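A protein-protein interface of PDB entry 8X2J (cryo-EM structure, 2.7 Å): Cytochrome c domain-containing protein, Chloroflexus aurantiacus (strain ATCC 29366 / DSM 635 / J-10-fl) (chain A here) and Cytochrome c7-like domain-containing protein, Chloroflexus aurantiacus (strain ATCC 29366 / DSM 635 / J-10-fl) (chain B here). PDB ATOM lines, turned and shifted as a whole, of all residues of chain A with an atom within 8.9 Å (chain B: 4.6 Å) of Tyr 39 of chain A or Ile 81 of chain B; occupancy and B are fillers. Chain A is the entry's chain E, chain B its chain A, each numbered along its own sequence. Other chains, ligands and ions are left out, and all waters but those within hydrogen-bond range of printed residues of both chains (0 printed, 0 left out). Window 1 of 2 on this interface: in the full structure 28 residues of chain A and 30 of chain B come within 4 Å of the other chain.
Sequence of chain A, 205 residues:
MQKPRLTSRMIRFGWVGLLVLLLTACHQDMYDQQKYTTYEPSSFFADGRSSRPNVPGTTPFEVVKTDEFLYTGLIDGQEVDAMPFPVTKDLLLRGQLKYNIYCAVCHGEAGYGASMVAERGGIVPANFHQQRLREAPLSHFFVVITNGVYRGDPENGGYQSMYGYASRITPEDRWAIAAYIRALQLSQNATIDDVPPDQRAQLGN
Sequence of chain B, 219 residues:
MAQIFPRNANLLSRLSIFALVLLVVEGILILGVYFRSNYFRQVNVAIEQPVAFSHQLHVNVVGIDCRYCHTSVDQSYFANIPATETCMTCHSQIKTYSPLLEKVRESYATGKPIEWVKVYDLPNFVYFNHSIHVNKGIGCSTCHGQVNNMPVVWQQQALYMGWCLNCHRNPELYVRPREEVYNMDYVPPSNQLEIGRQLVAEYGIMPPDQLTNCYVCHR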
ATOM      1  N   TYR A  36       7.717  -4.538   9.121  1.00  0.00           N
ATOM      2  CA  TYR A  36       6.927  -3.783   8.163  1.00  0.00           C
ATOM      3  C   TYR A  36       7.679  -3.680   6.845  1.00  0.00           C
ATOM      4  O   TYR A  36       8.851  -3.298   6.818  1.00  0.00           O
ATOM      5  CB  TYR A  36       6.596  -2.398   8.712  1.00  0.00           C
ATOM      6  CG  TYR A  36       5.421  -2.416   9.655  1.00  0.00           C
ATOM      7  CD1 TYR A  36       4.137  -2.645   9.182  1.00  0.00           C
ATOM      8  CD2 TYR A  36       5.596  -2.221  11.018  1.00  0.00           C
ATOM      9  CE1 TYR A  36       3.058  -2.671  10.036  1.00  0.00           C
ATOM     10  CE2 TYR A  36       4.518  -2.242  11.883  1.00  0.00           C
ATOM     11  CZ  TYR A  36       3.254  -2.467  11.385  1.00  0.00           C
ATOM     12  OH  TYR A  36       2.177  -2.492  12.235  1.00  0.00           O
ATOM     13  N   THR A  37       6.990  -4.006   5.754  1.00  0.00           N
ATOM     14  CA  THR A  37       7.578  -4.037   4.422  1.00  0.00           C
ATOM     15  C   THR A  37       7.425  -2.605   3.871  1.00  0.00           C
ATOM     16  O   THR A  37       7.126  -1.679   4.630  1.00  0.00           O
ATOM     17  CB  THR A  37       6.921  -5.190   3.648  1.00  0.00           C
ATOM     18  OG1 THR A  37       7.059  -6.376   4.434  1.00  0.00           O
ATOM     19  CG2 THR A  37       7.645  -5.553   2.340  1.00  0.00           C
ATOM     20  N   THR A  38       7.655  -2.376   2.570  1.00  0.00           N
ATOM     21  CA  THR A  38       7.731  -1.019   2.031  1.00  0.00           C
ATOM     22  C   THR A  38       6.385  -0.304   2.090  1.00  0.00           C
ATOM     23  O   THR A  38       6.285   0.798   2.641  1.00  0.00           O
ATOM     24  CB  THR A  38       8.254  -1.057   0.597  1.00  0.00           C
ATOM     25  OG1 THR A  38       9.569  -1.622   0.586  1.00  0.00           O
ATOM     26  CG2 THR A  38       8.312   0.342   0.016  1.00  0.00           C
ATOM     27  N   TYR A  39       5.332  -0.928   1.576  1.00  0.00           N
ATOM     28  CA  TYR A  39       4.010  -0.318   1.576  1.00  0.00           C
ATOM     29  C   TYR A  39       3.023  -1.137   2.401  1.00  0.00           C
ATOM     30  O   TYR A  39       1.845  -1.237   2.057  1.00  0.00           O
ATOM     31  CB  TYR A  39       3.500  -0.131   0.150  1.00  0.00           C
ATOM     32  CG  TYR A  39       4.049   1.080  -0.571  1.00  0.00           C
ATOM     33  CD1 TYR A  39       4.784   2.045   0.104  1.00  0.00           C
ATOM     34  CD2 TYR A  39       3.822   1.260  -1.927  1.00  0.00           C
ATOM     35  CE1 TYR A  39       5.283   3.150  -0.555  1.00  0.00           C
ATOM     36  CE2 TYR A  39       4.317   2.361  -2.592  1.00  0.00           C
ATOM     37  CZ  TYR A  39       5.045   3.302  -1.902  1.00  0.00           C
ATOM     38  OH  TYR A  39       5.537   4.401  -2.562  1.00  0.00           O
ATOM     39  N   GLU A  40       3.503  -1.735   3.483  1.00  0.00           N
ATOM     40  CA  GLU A  40       2.645  -2.526   4.358  1.00  0.00           C
ATOM     41  C   GLU A  40       1.730  -1.599   5.153  1.00  0.00           C
ATOM     42  O   GLU A  40       2.191  -0.570   5.654  1.00  0.00           O
ATOM     43  CB  GLU A  40       3.506  -3.373   5.296  1.00  0.00           C
ATOM     44  CG  GLU A  40       2.745  -4.358   6.167  1.00  0.00           C
ATOM     45  CD  GLU A  40       3.654  -5.395   6.800  1.00  0.00           C
ATOM     46  OE1 GLU A  40       4.746  -5.644   6.249  1.00  0.00           O
ATOM     47  OE2 GLU A  40       3.285  -5.963   7.848  1.00  0.00           O
ATOM     48  N   PRO A  41       0.436  -1.898   5.255  1.00  0.00           N
ATOM     49  CA  PRO A  41      -0.441  -1.079   6.096  1.00  0.00           C
ATOM     50  C   PRO A  41      -0.169  -1.306   7.575  1.00  0.00           C
ATOM     51  O   PRO A  41       0.266  -2.380   7.993  1.00  0.00           O
ATOM     52  CB  PRO A  41      -1.845  -1.551   5.709  1.00  0.00           C
ATOM     53  CG  PRO A  41      -1.647  -2.930   5.204  1.00  0.00           C
ATOM     54  CD  PRO A  41      -0.309  -2.944   4.536  1.00  0.00           C
ATOM     55  N   SER A  42      -0.434  -0.273   8.370  1.00  0.00           N
ATOM     56  CA  SER A  42      -0.188  -0.327   9.803  1.00  0.00           C
ATOM     57  C   SER A  42      -1.332   0.334  10.550  1.00  0.00           C
ATOM     58  O   SER A  42      -1.803   1.402  10.156  1.00  0.00           O
ATOM     59  CB  SER A  42       1.130   0.361  10.171  1.00  0.00           C
ATOM     60  OG  SER A  42       1.314   0.392  11.573  1.00  0.00           O
ATOM     61  N   GLY A  48      -3.232   4.981   8.563  1.00  0.00           N
ATOM     62  CA  GLY A  48      -3.262   3.573   8.209  1.00  0.00           C
ATOM     63  C   GLY A  48      -2.177   3.127   7.255  1.00  0.00           C
ATOM     64  O   GLY A  48      -2.456   2.371   6.315  1.00  0.00           O
ATOM     65  N   ARG A  49      -0.940   3.566   7.475  1.00  0.00           N
ATOM     66  CA  ARG A  49       0.147   3.289   6.543  1.00  0.00           C
ATOM     67  C   ARG A  49       1.463   3.321   7.301  1.00  0.00           C
ATOM     68  O   ARG A  49       1.749   4.297   7.999  1.00  0.00           O
ATOM     69  CB  ARG A  49       0.143   4.310   5.405  1.00  0.00           C
ATOM     70  CG  ARG A  49       1.322   4.231   4.469  1.00  0.00           C
ATOM     71  CD  ARG A  49       1.346   5.426   3.533  1.00  0.00           C
ATOM     72  NE  ARG A  49       0.007   5.874   3.172  1.00  0.00           N
ATOM     73  CZ  ARG A  49      -0.403   7.133   3.229  1.00  0.00           C
ATOM     74  NH1 ARG A  49       0.399   8.103   3.634  1.00  0.00           N
ATOM     75  NH2 ARG A  49      -1.647   7.427   2.870  1.00  0.00           N
ATOM     76  N   SER A  50       2.260   2.257   7.170  1.00  0.00           N
ATOM     77  CA  SER A  50       3.557   2.217   7.836  1.00  0.00           C
ATOM     78  C   SER A  50       4.599   3.067   7.127  1.00  0.00           C
ATOM     79  O   SER A  50       5.612   3.421   7.738  1.00  0.00           O
ATOM     80  CB  SER A  50       4.061   0.780   7.938  1.00  0.00           C
ATOM     81  OG  SER A  50       5.431   0.749   8.285  1.00  0.00           O
ATOM     82  N   SER A  51       4.382   3.389   5.856  1.00  0.00           N
ATOM     83  CA  SER A  51       5.295   4.260   5.128  1.00  0.00           C
ATOM     84  C   SER A  51       5.080   5.702   5.566  1.00  0.00           C
ATOM     85  O   SER A  51       3.977   6.241   5.434  1.00  0.00           O
ATOM     86  CB  SER A  51       5.074   4.112   3.628  1.00  0.00           C
ATOM     87  OG  SER A  51       5.723   2.958   3.133  1.00  0.00           O
ATOM     88  N   ARG A  52       6.132   6.326   6.077  1.00  0.00           N
ATOM     89  CA  ARG A  52       5.994   7.658   6.641  1.00  0.00           C
ATOM     90  C   ARG A  52       6.438   8.728   5.657  1.00  0.00           C
ATOM     91  O   ARG A  52       7.411   8.530   4.926  1.00  0.00           O
ATOM     92  CB  ARG A  52       6.808   7.776   7.932  1.00  0.00           C
ATOM     93  CG  ARG A  52       6.318   6.915   9.100  1.00  0.00           C
ATOM     94  CD  ARG A  52       4.962   7.387   9.628  1.00  0.00           C
ATOM     95  NE  ARG A  52       3.819   6.802   8.937  1.00  0.00           N
ATOM     96  CZ  ARG A  52       2.579   7.258   9.026  1.00  0.00           C
ATOM     97  NH1 ARG A  52       2.284   8.323   9.751  1.00  0.00           N
ATOM     98  NH2 ARG A  52       1.614   6.639   8.356  1.00  0.00           N
ATOM     99  N   CYS B  69       4.113   4.799 -13.370  1.00  0.00           N
ATOM    100  CA  CYS B  69       3.421   4.393 -12.160  1.00  0.00           C
ATOM    101  C   CYS B  69       4.271   3.512 -11.258  1.00  0.00           C
ATOM    102  O   CYS B  69       4.246   3.682 -10.037  1.00  0.00           O
ATOM    103  CB  CYS B  69       2.129   3.677 -12.541  1.00  0.00           C
ATOM    104  SG  CYS B  69       0.858   4.808 -13.137  1.00  0.00           S
ATOM    105  N   PHE B  78      11.807  -2.824  -4.889  1.00  0.00           N
ATOM    106  CA  PHE B  78      10.364  -2.679  -4.816  1.00  0.00           C
ATOM    107  C   PHE B  78       9.880  -1.888  -6.022  1.00  0.00           C
ATOM    108  O   PHE B  78      10.234  -0.717  -6.183  1.00  0.00           O
ATOM    109  CB  PHE B  78       9.976  -1.981  -3.512  1.00  0.00           C
ATOM    110  CG  PHE B  78       8.500  -1.924  -3.265  1.00  0.00           C
ATOM    111  CD1 PHE B  78       7.813  -3.043  -2.828  1.00  0.00           C
ATOM    112  CD2 PHE B  78       7.805  -0.742  -3.451  1.00  0.00           C
ATOM    113  CE1 PHE B  78       6.455  -2.988  -2.596  1.00  0.00           C
ATOM    114  CE2 PHE B  78       6.449  -0.683  -3.222  1.00  0.00           C
ATOM    115  CZ  PHE B  78       5.773  -1.806  -2.794  1.00  0.00           C
ATOM    116  N   ALA B  79       9.095  -2.536  -6.875  1.00  0.00           N
ATOM    117  CA  ALA B  79       8.358  -1.807  -7.895  1.00  0.00           C
ATOM    118  C   ALA B  79       7.284  -0.975  -7.215  1.00  0.00           C
ATOM    119  O   ALA B  79       6.570  -1.466  -6.337  1.00  0.00           O
ATOM    120  CB  ALA B  79       7.735  -2.769  -8.899  1.00  0.00           C
ATOM    121  N   ASN B  80       7.167   0.282  -7.620  1.00  0.00           N
ATOM    122  CA  ASN B  80       6.350   1.242  -6.892  1.00  0.00           C
ATOM    123  C   ASN B  80       4.870   0.982  -7.140  1.00  0.00           C
ATOM    124  O   ASN B  80       4.413   0.993  -8.286  1.00  0.00           O
ATOM    125  CB  ASN B  80       6.723   2.661  -7.310  1.00  0.00           C
ATOM    126  CG  ASN B  80       6.233   3.699  -6.337  1.00  0.00           C
ATOM    127  OD1 ASN B  80       5.918   3.389  -5.194  1.00  0.00           O
ATOM    128  ND2 ASN B  80       6.161   4.943  -6.786  1.00  0.00           N
ATOM    129  N   ILE B  81       4.127   0.723  -6.074  1.00  0.00           N
ATOM    130  CA  ILE B  81       2.670   0.845  -6.162  1.00  0.00           C
ATOM    131  C   ILE B  81       2.317   2.328  -6.211  1.00  0.00           C
ATOM    132  O   ILE B  81       2.768   3.091  -5.338  1.00  0.00           O
ATOM    133  CB  ILE B  81       2.002   0.145  -4.974  1.00  0.00           C
ATOM    134  CG1 ILE B  81       2.317  -1.352  -4.996  1.00  0.00           C
ATOM    135  CG2 ILE B  81       0.495   0.352  -4.984  1.00  0.00           C
ATOM    136  CD1 ILE B  81       1.725  -2.084  -6.179  1.00  0.00           C
ATOM    137  N   PRO B  82       1.562   2.783  -7.209  1.00  0.00           N
ATOM    138  CA  PRO B  82       1.408   4.226  -7.437  1.00  0.00           C
ATOM    139  C   PRO B  82       0.586   4.916  -6.362  1.00  0.00           C
ATOM    140  O   PRO B  82      -0.179   4.301  -5.616  1.00  0.00           O
ATOM    141  CB  PRO B  82       0.692   4.305  -8.788  1.00  0.00           C
ATOM    142  CG  PRO B  82       0.704   2.948  -9.324  1.00  0.00           C
ATOM    143  CD  PRO B  82       0.859   1.992  -8.224  1.00  0.00           C
ATOM    144  N   ALA B  83       0.762   6.227  -6.302  1.00  0.00           N
ATOM    145  CA  ALA B  83       0.086   7.056  -5.324  1.00  0.00           C
ATOM    146  C   ALA B  83      -1.224   7.599  -5.881  1.00  0.00           C
ATOM    147  O   ALA B  83      -1.461   7.625  -7.096  1.00  0.00           O
ATOM    148  CB  ALA B  83       0.985   8.210  -4.887  1.00  0.00           C
ATOM    149  N   TRP B 116      -4.909  -1.688  -2.078  1.00  0.00           N
ATOM    150  CA  TRP B 116      -4.843  -2.694  -3.124  1.00  0.00           C
ATOM    151  C   TRP B 116      -4.439  -4.041  -2.533  1.00  0.00           C
ATOM    152  O   TRP B 116      -3.830  -4.124  -1.463  1.00  0.00           O
ATOM    153  CB  TRP B 116      -3.838  -2.304  -4.209  1.00  0.00           C
ATOM    154  CG  TRP B 116      -3.935  -0.905  -4.729  1.00  0.00           C
ATOM    155  CD1 TRP B 116      -3.139   0.148  -4.391  1.00  0.00           C
ATOM    156  CD2 TRP B 116      -4.853  -0.413  -5.712  1.00  0.00           C
ATOM    157  NE1 TRP B 116      -3.514   1.268  -5.087  1.00  0.00           N
ATOM    158  CE2 TRP B 116      -4.564   0.950  -5.906  1.00  0.00           C
ATOM    159  CE3 TRP B 116      -5.901  -0.989  -6.435  1.00  0.00           C
ATOM    160  CZ2 TRP B 116      -5.280   1.744  -6.796  1.00  0.00           C
ATOM    161  CZ3 TRP B 116      -6.606  -0.201  -7.320  1.00  0.00           C
ATOM    162  CH2 TRP B 116      -6.293   1.150  -7.493  1.00  0.00           C
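The side-chain amide oxygen (OD1) of Asn 80 of chain B is in hydrogen-bond range of the side-chain hydroxyl (OH) of Tyr 39 of chain A (2.8 Å).
Among the printed residues, merely in contact across the chains: Tyr 39 of chain A with Ile 81 of chain B, Tyr 39 of chain A with Phe 78 of chain B and Thr 38 of chain A with Phe 78 of chain B.
Of the printed residues of chain B, Thr 38 of chain A touches Phe 78 (3.7 Å). Of chain B, only Phe 78, Asn 80 and Ile 81 come within 4 Å of Tyr 39 of chain A. Printed residues of chain A within 4 Å of Phe 78 of chain B: Thr 38 and Tyr 39. Of chain A, only Tyr 39 (3.2 Å) comes within 4 Å of Ile 81 of chain B. No residue of chain A comes within 4 Å of Pro 82 of chain B. The nearest printed residue of chain B that does not touch Tyr 39 of chain A is Pro 82 of chain B (5.4 Å).
Hydrophobic or aromatic side chains of chain A within 4 Å of the printed part of chain B: Tyr 39. Along chain A the printed residues that touch a printed residue of chain B span positions 38 to 39. Among the printed residues, no Asp or Glu carboxylate lies within 4 Å of a Lys or Arg side-chain nitrogen of the other chain.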
